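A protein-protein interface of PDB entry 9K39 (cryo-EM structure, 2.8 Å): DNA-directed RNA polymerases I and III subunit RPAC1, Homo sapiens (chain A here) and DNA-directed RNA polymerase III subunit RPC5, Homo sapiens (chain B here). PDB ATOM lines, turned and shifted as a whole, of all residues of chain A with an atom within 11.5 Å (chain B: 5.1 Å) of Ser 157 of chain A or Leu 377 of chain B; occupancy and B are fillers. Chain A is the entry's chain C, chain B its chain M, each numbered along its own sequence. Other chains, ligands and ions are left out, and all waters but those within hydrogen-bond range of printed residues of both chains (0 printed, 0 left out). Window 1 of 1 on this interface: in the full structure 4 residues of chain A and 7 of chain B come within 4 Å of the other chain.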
ATOM      1  N   ARG A 148      28.951 -25.458  -8.128  1.00  0.00           N
ATOM      2  CA  ARG A 148      28.989 -24.422  -7.108  1.00  0.00           C
ATOM      3  C   ARG A 148      29.507 -23.110  -7.688  1.00  0.00           C
ATOM      4  O   ARG A 148      30.373 -23.089  -8.567  1.00  0.00           O
ATOM      5  CB  ARG A 148      29.869 -24.857  -5.936  1.00  0.00           C
ATOM      6  CG  ARG A 148      29.431 -26.157  -5.279  1.00  0.00           C
ATOM      7  CD  ARG A 148      30.365 -26.545  -4.144  1.00  0.00           C
ATOM      8  NE  ARG A 148      29.986 -27.816  -3.533  1.00  0.00           N
ATOM      9  CZ  ARG A 148      29.151 -27.930  -2.506  1.00  0.00           C
ATOM     10  NH1 ARG A 148      28.604 -26.849  -1.969  1.00  0.00           N
ATOM     11  NH2 ARG A 148      28.861 -29.127  -2.014  1.00  0.00           N
ATOM     12  N   ASN A 149      28.963 -22.010  -7.186  1.00  0.00           N
ATOM     13  CA  ASN A 149      29.383 -20.685  -7.630  1.00  0.00           C
ATOM     14  C   ASN A 149      30.758 -20.360  -7.059  1.00  0.00           C
ATOM     15  O   ASN A 149      30.921 -20.362  -5.831  1.00  0.00           O
ATOM     16  CB  ASN A 149      28.361 -19.636  -7.202  1.00  0.00           C
ATOM     17  CG  ASN A 149      28.650 -18.265  -7.784  1.00  0.00           C
ATOM     18  OD1 ASN A 149      29.319 -18.142  -8.807  1.00  0.00           O
ATOM     19  ND2 ASN A 149      28.141 -17.229  -7.130  1.00  0.00           N
ATOM     20  N   HIS A 151      32.233 -17.591  -6.679  1.00  0.00           N
ATOM     21  CA  HIS A 151      32.198 -16.354  -5.907  1.00  0.00           C
ATOM     22  C   HIS A 151      30.820 -16.221  -5.268  1.00  0.00           C
ATOM     23  O   HIS A 151      29.830 -15.981  -5.967  1.00  0.00           O
ATOM     24  CB  HIS A 151      32.515 -15.144  -6.786  1.00  0.00           C
ATOM     25  CG  HIS A 151      33.892 -15.169  -7.375  1.00  0.00           C
ATOM     26  ND1 HIS A 151      34.279 -16.083  -8.330  1.00  0.00           N
ATOM     27  CD2 HIS A 151      34.974 -14.388  -7.141  1.00  0.00           C
ATOM     28  CE1 HIS A 151      35.539 -15.867  -8.661  1.00  0.00           C
ATOM     29  NE2 HIS A 151      35.985 -14.843  -7.953  1.00  0.00           N
ATOM     30  N   ALA A 152      30.760 -16.371  -3.948  1.00  0.00           N
ATOM     31  CA  ALA A 152      29.505 -16.271  -3.219  1.00  0.00           C
ATOM     32  C   ALA A 152      29.791 -15.823  -1.795  1.00  0.00           C
ATOM     33  O   ALA A 152      30.939 -15.812  -1.343  1.00  0.00           O
ATOM     34  CB  ALA A 152      28.742 -17.601  -3.225  1.00  0.00           C
ATOM     35  N   ALA A 153      28.725 -15.454  -1.088  1.00  0.00           N
ATOM     36  CA  ALA A 153      28.857 -15.009   0.289  1.00  0.00           C
ATOM     37  C   ALA A 153      29.243 -16.172   1.198  1.00  0.00           C
ATOM     38  O   ALA A 153      29.203 -17.344   0.810  1.00  0.00           O
ATOM     39  CB  ALA A 153      27.555 -14.373   0.777  1.00  0.00           C
ATOM     40  N   LYS A 154      29.629 -15.832   2.430  1.00  0.00           N
ATOM     41  CA  LYS A 154      30.020 -16.857   3.391  1.00  0.00           C
ATOM     42  C   LYS A 154      28.836 -17.740   3.770  1.00  0.00           C
ATOM     43  O   LYS A 154      28.966 -18.969   3.833  1.00  0.00           O
ATOM     44  CB  LYS A 154      30.626 -16.204   4.634  1.00  0.00           C
ATOM     45  CG  LYS A 154      31.757 -15.235   4.330  1.00  0.00           C
ATOM     46  CD  LYS A 154      32.880 -15.918   3.566  1.00  0.00           C
ATOM     47  CE  LYS A 154      33.978 -14.932   3.202  1.00  0.00           C
ATOM     48  NZ  LYS A 154      33.467 -13.829   2.340  1.00  0.00           N
ATOM     49  N   ASP A 155      27.678 -17.133   4.025  1.00  0.00           N
ATOM     50  CA  ASP A 155      26.492 -17.908   4.372  1.00  0.00           C
ATOM     51  C   ASP A 155      25.804 -18.457   3.126  1.00  0.00           C
ATOM     52  O   ASP A 155      25.727 -19.674   2.931  1.00  0.00           O
ATOM     53  CB  ASP A 155      25.527 -17.049   5.194  1.00  0.00           C
ATOM     54  CG  ASP A 155      25.368 -15.649   4.628  1.00  0.00           C
ATOM     55  OD1 ASP A 155      26.053 -15.327   3.635  1.00  0.00           O
ATOM     56  OD2 ASP A 155      24.559 -14.872   5.178  1.00  0.00           O
ATOM     57  N   SER A 156      25.318 -17.565   2.263  1.00  0.00           N
ATOM     58  CA  SER A 156      24.633 -17.921   1.023  1.00  0.00           C
ATOM     59  C   SER A 156      23.532 -18.954   1.271  1.00  0.00           C
ATOM     60  O   SER A 156      23.557 -20.073   0.755  1.00  0.00           O
ATOM     61  CB  SER A 156      25.635 -18.422  -0.023  1.00  0.00           C
ATOM     62  OG  SER A 156      26.596 -17.424  -0.325  1.00  0.00           O
ATOM     63  N   SER A 157      22.555 -18.553   2.087  1.00  0.00           N
ATOM     64  CA  SER A 157      21.461 -19.459   2.425  1.00  0.00           C
ATOM     65  C   SER A 157      20.587 -19.750   1.212  1.00  0.00           C
ATOM     66  O   SER A 157      20.087 -20.871   1.053  1.00  0.00           O
ATOM     67  CB  SER A 157      20.625 -18.869   3.563  1.00  0.00           C
ATOM     68  OG  SER A 157      19.558 -19.734   3.913  1.00  0.00           O
ATOM     69  N   ASP A 158      20.387 -18.759   0.352  1.00  0.00           N
ATOM     70  CA  ASP A 158      19.563 -18.962  -0.829  1.00  0.00           C
ATOM     71  C   ASP A 158      20.309 -19.813  -1.854  1.00  0.00           C
ATOM     72  O   ASP A 158      21.505 -19.604  -2.085  1.00  0.00           O
ATOM     73  CB  ASP A 158      19.170 -17.619  -1.447  1.00  0.00           C
ATOM     74  CG  ASP A 158      20.372 -16.754  -1.772  1.00  0.00           C
ATOM     75  OD1 ASP A 158      21.392 -16.861  -1.057  1.00  0.00           O
ATOM     76  OD2 ASP A 158      20.295 -15.968  -2.738  1.00  0.00           O
ATOM     77  N   PRO A 159      19.639 -20.786  -2.476  1.00  0.00           N
ATOM     78  CA  PRO A 159      20.320 -21.622  -3.476  1.00  0.00           C
ATOM     79  C   PRO A 159      20.756 -20.858  -4.715  1.00  0.00           C
ATOM     80  O   PRO A 159      21.611 -21.358  -5.460  1.00  0.00           O
ATOM     81  CB  PRO A 159      19.270 -22.689  -3.821  1.00  0.00           C
ATOM     82  CG  PRO A 159      18.305 -22.672  -2.675  1.00  0.00           C
ATOM     83  CD  PRO A 159      18.269 -21.251  -2.209  1.00  0.00           C
ATOM     84  N   ASN A 160      20.197 -19.671  -4.963  1.00  0.00           N
ATOM     85  CA  ASN A 160      20.576 -18.908  -6.148  1.00  0.00           C
ATOM     86  C   ASN A 160      22.026 -18.444  -6.070  1.00  0.00           C
ATOM     87  O   ASN A 160      22.751 -18.473  -7.069  1.00  0.00           O
ATOM     88  CB  ASN A 160      19.638 -17.712  -6.322  1.00  0.00           C
ATOM     89  CG  ASN A 160      18.186 -18.126  -6.448  1.00  0.00           C
ATOM     90  OD1 ASN A 160      17.363 -17.801  -5.593  1.00  0.00           O
ATOM     91  ND2 ASN A 160      17.865 -18.845  -7.517  1.00  0.00           N
ATOM     92  N   GLU A 161      22.466 -18.006  -4.886  1.00  0.00           N
ATOM     93  CA  GLU A 161      23.831 -17.508  -4.748  1.00  0.00           C
ATOM     94  C   GLU A 161      24.832 -18.653  -4.641  1.00  0.00           C
ATOM     95  O   GLU A 161      25.960 -18.545  -5.138  1.00  0.00           O
ATOM     96  CB  GLU A 161      23.929 -16.589  -3.528  1.00  0.00           C
ATOM     97  CG  GLU A 161      25.256 -15.854  -3.414  1.00  0.00           C
ATOM     98  CD  GLU A 161      25.292 -14.900  -2.237  1.00  0.00           C
ATOM     99  OE1 GLU A 161      24.405 -14.993  -1.361  1.00  0.00           O
ATOM    100  OE2 GLU A 161      26.208 -14.052  -2.189  1.00  0.00           O
ATOM    101  N   LEU A 162      24.440 -19.756  -3.999  1.00  0.00           N
ATOM    102  CA  LEU A 162      25.369 -20.863  -3.805  1.00  0.00           C
ATOM    103  C   LEU A 162      25.661 -21.592  -5.113  1.00  0.00           C
ATOM    104  O   LEU A 162      26.818 -21.915  -5.403  1.00  0.00           O
ATOM    105  CB  LEU A 162      24.816 -21.844  -2.770  1.00  0.00           C
ATOM    106  CG  LEU A 162      25.386 -21.755  -1.355  1.00  0.00           C
ATOM    107  CD1 LEU A 162      24.815 -22.855  -0.475  1.00  0.00           C
ATOM    108  CD2 LEU A 162      26.905 -21.816  -1.381  1.00  0.00           C
ATOM    109  N   TYR A 163      24.631 -21.859  -5.909  1.00  0.00           N
ATOM    110  CA  TYR A 163      24.763 -22.692  -7.092  1.00  0.00           C
ATOM    111  C   TYR A 163      24.345 -21.921  -8.339  1.00  0.00           C
ATOM    112  O   TYR A 163      23.615 -20.931  -8.271  1.00  0.00           O
ATOM    113  CB  TYR A 163      23.923 -23.969  -6.961  1.00  0.00           C
ATOM    114  CG  TYR A 163      23.871 -24.510  -5.550  1.00  0.00           C
ATOM    115  CD1 TYR A 163      24.982 -25.108  -4.974  1.00  0.00           C
ATOM    116  CD2 TYR A 163      22.708 -24.420  -4.795  1.00  0.00           C
ATOM    117  CE1 TYR A 163      24.938 -25.605  -3.683  1.00  0.00           C
ATOM    118  CE2 TYR A 163      22.656 -24.915  -3.504  1.00  0.00           C
ATOM    119  CZ  TYR A 163      23.773 -25.505  -2.955  1.00  0.00           C
ATOM    120  OH  TYR A 163      23.724 -25.997  -1.670  1.00  0.00           O
ATOM    121  N   HIS A 166      21.068 -24.263 -11.261  1.00  0.00           N
ATOM    122  CA  HIS A 166      20.413 -25.241 -10.404  1.00  0.00           C
ATOM    123  C   HIS A 166      18.964 -25.489 -10.798  1.00  0.00           C
ATOM    124  O   HIS A 166      18.402 -26.520 -10.417  1.00  0.00           O
ATOM    125  CB  HIS A 166      20.481 -24.792  -8.943  1.00  0.00           C
ATOM    126  CG  HIS A 166      19.778 -23.498  -8.673  1.00  0.00           C
ATOM    127  ND1 HIS A 166      20.279 -22.281  -9.086  1.00  0.00           N
ATOM    128  CD2 HIS A 166      18.619 -23.229  -8.028  1.00  0.00           C
ATOM    129  CE1 HIS A 166      19.455 -21.319  -8.710  1.00  0.00           C
ATOM    130  NE2 HIS A 166      18.440 -21.867  -8.065  1.00  0.00           N
ATOM    131  N   LYS A 167      18.351 -24.576 -11.547  1.00  0.00           N
ATOM    132  CA  LYS A 167      16.988 -24.737 -12.048  1.00  0.00           C
ATOM    133  C   LYS A 167      17.053 -24.788 -13.569  1.00  0.00           C
ATOM    134  O   LYS A 167      17.346 -23.777 -14.216  1.00  0.00           O
ATOM    135  CB  LYS A 167      16.086 -23.600 -11.573  1.00  0.00           C
ATOM    136  CG  LYS A 167      15.838 -23.577 -10.074  1.00  0.00           C
ATOM    137  CD  LYS A 167      14.946 -22.409  -9.685  1.00  0.00           C
ATOM    138  CE  LYS A 167      14.672 -22.390  -8.188  1.00  0.00           C
ATOM    139  NZ  LYS A 167      13.963 -23.619  -7.738  1.00  0.00           N
ATOM    140  N   GLN A 201      15.018 -29.254 -11.073  1.00  0.00           N
ATOM    141  CA  GLN A 201      15.929 -28.525 -10.205  1.00  0.00           C
ATOM    142  C   GLN A 201      17.116 -29.419  -9.877  1.00  0.00           C
ATOM    143  O   GLN A 201      16.948 -30.606  -9.588  1.00  0.00           O
ATOM    144  CB  GLN A 201      15.231 -28.068  -8.920  1.00  0.00           C
ATOM    145  CG  GLN A 201      15.987 -26.998  -8.149  1.00  0.00           C
ATOM    146  CD  GLN A 201      15.213 -26.489  -6.948  1.00  0.00           C
ATOM    147  OE1 GLN A 201      14.062 -26.865  -6.734  1.00  0.00           O
ATOM    148  NE2 GLN A 201      15.845 -25.627  -6.161  1.00  0.00           N
ATOM    149  N   ARG A 203      21.432 -29.901  -8.360  1.00  0.00           N
ATOM    150  CA  ARG A 203      22.397 -29.663  -7.299  1.00  0.00           C
ATOM    151  C   ARG A 203      23.795 -29.823  -7.876  1.00  0.00           C
ATOM    152  O   ARG A 203      23.967 -30.447  -8.931  1.00  0.00           O
ATOM    153  CB  ARG A 203      22.186 -30.639  -6.132  1.00  0.00           C
ATOM    154  CG  ARG A 203      21.024 -30.268  -5.225  1.00  0.00           C
ATOM    155  CD  ARG A 203      21.281 -28.942  -4.527  1.00  0.00           C
ATOM    156  NE  ARG A 203      20.139 -28.513  -3.725  1.00  0.00           N
ATOM    157  CZ  ARG A 203      19.188 -27.691  -4.159  1.00  0.00           C
ATOM    158  NH1 ARG A 203      19.241 -27.205  -5.392  1.00  0.00           N
ATOM    159  NH2 ARG A 203      18.184 -27.355  -3.361  1.00  0.00           N
ATOM    160  N   PRO A 204      24.812 -29.257  -7.225  1.00  0.00           N
ATOM    161  CA  PRO A 204      26.178 -29.388  -7.753  1.00  0.00           C
ATOM    162  C   PRO A 204      26.601 -30.849  -7.840  1.00  0.00           C
ATOM    163  O   PRO A 204      26.426 -31.625  -6.900  1.00  0.00           O
ATOM    164  CB  PRO A 204      27.029 -28.608  -6.743  1.00  0.00           C
ATOM    165  CG  PRO A 204      26.187 -28.521  -5.511  1.00  0.00           C
ATOM    166  CD  PRO A 204      24.778 -28.436  -6.005  1.00  0.00           C
ATOM    167  N   SER B 342      17.941 -24.623   7.089  1.00  0.00           N
ATOM    168  CA  SER B 342      19.009 -24.489   6.109  1.00  0.00           C
ATOM    169  C   SER B 342      20.358 -25.012   6.581  1.00  0.00           C
ATOM    170  O   SER B 342      21.220 -25.280   5.735  1.00  0.00           O
ATOM    171  CB  SER B 342      19.175 -23.019   5.690  1.00  0.00           C
ATOM    172  OG  SER B 342      19.486 -22.201   6.805  1.00  0.00           O
ATOM    173  N   VAL B 344      22.654 -23.363   8.247  1.00  0.00           N
ATOM    174  CA  VAL B 344      23.661 -22.307   8.302  1.00  0.00           C
ATOM    175  C   VAL B 344      24.119 -22.145   9.747  1.00  0.00           C
ATOM    176  O   VAL B 344      23.375 -22.501  10.672  1.00  0.00           O
ATOM    177  CB  VAL B 344      23.115 -20.988   7.731  1.00  0.00           C
ATOM    178  CG1 VAL B 344      22.687 -21.176   6.282  1.00  0.00           C
ATOM    179  CG2 VAL B 344      21.957 -20.480   8.572  1.00  0.00           C
ATOM    180  N   VAL B 348      25.241 -16.436  11.591  1.00  0.00           N
ATOM    181  CA  VAL B 348      24.466 -15.785  10.538  1.00  0.00           C
ATOM    182  C   VAL B 348      23.033 -15.558  10.995  1.00  0.00           C
ATOM    183  O   VAL B 348      22.430 -14.519  10.699  1.00  0.00           O
ATOM    184  CB  VAL B 348      24.527 -16.617   9.244  1.00  0.00           C
ATOM    185  CG1 VAL B 348      23.753 -15.926   8.138  1.00  0.00           C
ATOM    186  CG2 VAL B 348      25.972 -16.850   8.832  1.00  0.00           C
ATOM    187  N   GLY B 352      21.229 -11.939  11.253  1.00  0.00           N
ATOM    188  CA  GLY B 352      19.952 -11.655  10.617  1.00  0.00           C
ATOM    189  C   GLY B 352      18.898 -11.191  11.604  1.00  0.00           C
ATOM    190  O   GLY B 352      18.140 -10.259  11.324  1.00  0.00           O
ATOM    191  N   ALA B 372      14.999 -10.300   3.150  1.00  0.00           N
ATOM    192  CA  ALA B 372      15.530 -11.452   2.429  1.00  0.00           C
ATOM    193  C   ALA B 372      16.624 -11.037   1.453  1.00  0.00           C
ATOM    194  O   ALA B 372      17.603 -11.768   1.258  1.00  0.00           O
ATOM    195  CB  ALA B 372      14.402 -12.179   1.698  1.00  0.00           C
ATOM    196  N   THR B 375      19.834  -9.639   3.885  1.00  0.00           N
ATOM    197  CA  THR B 375      20.482 -10.692   4.655  1.00  0.00           C
ATOM    198  C   THR B 375      20.897 -11.886   3.806  1.00  0.00           C
ATOM    199  O   THR B 375      21.622 -12.753   4.307  1.00  0.00           O
ATOM    200  CB  THR B 375      19.558 -11.168   5.778  1.00  0.00           C
ATOM    201  OG1 THR B 375      18.335 -11.663   5.216  1.00  0.00           O
ATOM    202  CG2 THR B 375      19.246 -10.023   6.731  1.00  0.00           C
ATOM    203  N   LYS B 376      20.451 -11.955   2.550  1.00  0.00           N
ATOM    204  CA  LYS B 376      20.766 -13.053   1.637  1.00  0.00           C
ATOM    205  C   LYS B 376      20.332 -14.408   2.186  1.00  0.00           C
ATOM    206  O   LYS B 376      20.882 -15.444   1.795  1.00  0.00           O
ATOM    207  CB  LYS B 376      22.260 -13.078   1.290  1.00  0.00           C
ATOM    208  CG  LYS B 376      22.776 -11.798   0.656  1.00  0.00           C
ATOM    209  CD  LYS B 376      22.090 -11.522  -0.671  1.00  0.00           C
ATOM    210  CE  LYS B 376      22.636 -10.262  -1.324  1.00  0.00           C
ATOM    211  NZ  LYS B 376      21.984  -9.986  -2.633  1.00  0.00           N
ATOM    212  N   LEU B 377      19.353 -14.423   3.085  1.00  0.00           N
ATOM    213  CA  LEU B 377      18.881 -15.653   3.699  1.00  0.00           C
ATOM    214  C   LEU B 377      17.684 -16.213   2.936  1.00  0.00           C
ATOM    215  O   LEU B 377      17.063 -15.536   2.114  1.00  0.00           O
ATOM    216  CB  LEU B 377      18.504 -15.416   5.161  1.00  0.00           C
ATOM    217  CG  LEU B 377      19.647 -15.018   6.095  1.00  0.00           C
ATOM    218  CD1 LEU B 377      19.139 -14.840   7.517  1.00  0.00           C
ATOM    219  CD2 LEU B 377      20.757 -16.054   6.044  1.00  0.00           C
ATOM    220  N   CYS B 378      17.369 -17.472   3.223  1.00  0.00           N
ATOM    221  CA  CYS B 378      16.232 -18.123   2.596  1.00  0.00           C
ATOM    222  C   CYS B 378      14.921 -17.597   3.177  1.00  0.00           C
ATOM    223  O   CYS B 378      14.898 -16.864   4.170  1.00  0.00           O
ATOM    224  CB  CYS B 378      16.319 -19.639   2.769  1.00  0.00           C
ATOM    225  SG  CYS B 378      16.603 -20.175   4.470  1.00  0.00           S
ATOM    226  N   ALA B 379      13.818 -17.985   2.537  1.00  0.00           N
ATOM    227  CA  ALA B 379      12.510 -17.475   2.940  1.00  0.00           C
ATOM    228  C   ALA B 379      12.098 -18.008   4.309  1.00  0.00           C
ATOM    229  O   ALA B 379      11.492 -17.281   5.106  1.00  0.00           O
ATOM    230  CB  ALA B 379      11.461 -17.834   1.888  1.00  0.00           C
ATOM    231  N   ASP B 381      13.950 -18.940   6.952  1.00  0.00           N
ATOM    232  CA  ASP B 381      14.646 -18.328   8.079  1.00  0.00           C
ATOM    233  C   ASP B 381      14.108 -16.931   8.368  1.00  0.00           C
ATOM    234  O   ASP B 381      13.905 -16.568   9.533  1.00  0.00           O
ATOM    235  CB  ASP B 381      16.150 -18.280   7.811  1.00  0.00           C
ATOM    236  CG  ASP B 381      16.803 -19.644   7.915  1.00  0.00           C
ATOM    237  OD1 ASP B 381      16.216 -20.538   8.559  1.00  0.00           O
ATOM    238  OD2 ASP B 381      17.906 -19.821   7.357  1.00  0.00           O
ATOM    239  N   VAL B 382      13.858 -16.140   7.323  1.00  0.00           N
ATOM    240  CA  VAL B 382      13.285 -14.811   7.518  1.00  0.00           C
ATOM    241  C   VAL B 382      11.877 -14.920   8.090  1.00  0.00           C
ATOM    242  O   VAL B 382      11.473 -14.122   8.945  1.00  0.00           O
ATOM    243  CB  VAL B 382      13.303 -14.023   6.195  1.00  0.00           C
ATOM    244  CG1 VAL B 382      12.718 -12.632   6.394  1.00  0.00           C
ATOM    245  CG2 VAL B 382      14.721 -13.935   5.650  1.00  0.00           C
ATOM    246  N   PHE B 385      12.223 -15.676  11.723  1.00  0.00           N
ATOM    247  CA  PHE B 385      12.667 -14.476  12.428  1.00  0.00           C
ATOM    248  C   PHE B 385      11.518 -13.496  12.629  1.00  0.00           C
ATOM    249  O   PHE B 385      11.408 -12.864  13.686  1.00  0.00           O
ATOM    250  CB  PHE B 385      13.810 -13.807  11.664  1.00  0.00           C
ATOM    251  CG  PHE B 385      15.087 -14.597  11.659  1.00  0.00           C
ATOM    252  CD1 PHE B 385      15.351 -15.522  12.656  1.00  0.00           C
ATOM    253  CD2 PHE B 385      16.027 -14.407  10.661  1.00  0.00           C
ATOM    254  CE1 PHE B 385      16.527 -16.247  12.652  1.00  0.00           C
ATOM    255  CE2 PHE B 385      17.206 -15.127  10.654  1.00  0.00           C
ATOM    256  CZ  PHE B 385      17.456 -16.049  11.650  1.00  0.00           C
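Printed residues of chain B that touch a printed residue of chain A: Ser 342, Val 348, Thr 375, Lys 376, Leu 377, Cys 378 and Asp 381. Hydrophobic or aromatic side chains of chain B that line the printed part of chain A: Val 348 and Leu 377. Along chain B the printed residues that touch a printed residue of chain A span positions 342 to 381. Among the printed residues, 9 pairs touch across the chains.
OG of Ser 342 of chain B is in hydrogen-bond range of OD2 of Asp 381 of chain B (2.9 Å). The side-chain carboxylate of Asp 381 of chain B is in hydrogen-bond range of the side-chain sulfur of Cys 378 of chain B (3.2 Å). ND2 of Asn 149 of chain A lies within hydrogen-bond range of O of Glu 161 of chain A, at 3.2 Å. N of Ala 153 of chain A is in hydrogen-bond range of OE2 of Glu 161 of chain A, at 3.1 Å. The side-chain carboxylate (OE1) of Glu 161 of chain A sits close to the side-chain hydroxyl (OG) of Ser 156 of chain A.
OG of Ser 157 of chain A lies within hydrogen-bond range of SG of Cys 378 of chain B (3.0 Å). OD1 of Asp 158 of chain A sits close to O of Lys 376 of chain B (3.2 Å).
Among the printed residues, pairs that only touch across the chains: Asp 155 of chain A with Val 348 of chain B, Asp 155 of chain A with Thr 375 of chain B, Ser 157 of chain A with Ser 342 of chain B, Ser 157 of chain A with Lys 376 of chain B, Ser 157 of chain A with Leu 377 of chain B, Ser 157 of chain A with Asp 381 of chain B and Glu 161 of chain A with Lys 376 of chain B.
Of the printed residues of chain B, Asp 155 of chain A touches Val 348 and Thr 375. Ser 157 of chain A touches just these residues of chain B: Ser 342 (3.8 Å), Lys 376 (3.5 Å), Leu 377 (3.7 Å), Cys 378 (3.0 Å) and Asp 381 (3.8 Å). Of the printed residues of chain B, Glu 161 of chain A touches Lys 376. Printed residues of chain A within 4 Å of Val 348 of chain B: Asp 155. No residue of chain A comes within 4 Å of Gly 352 of chain B. Of the printed residues of chain A, Thr 375 of chain B touches Asp 155 (3.7 Å). Leu 377 of chain B touches just one residue of chain A: Ser 157 (3.7 Å). No residue of chain A comes within 4 Å of Ala 379 of chain B. Asp 381 of chain B touches just one residue of chain A: Ser 157. The nearest residue of chain B that does not touch Ser 157 of chain A is Val 344 of chain B (4.1 Å). The nearest residue of chain A that does not touch Leu 377 of chain B is Asp 155 of chain A (4.1 Å). The nearest printed residue of chain B that does not touch Asp 158 of chain A is Cys 378 of chain B (4.4 Å).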
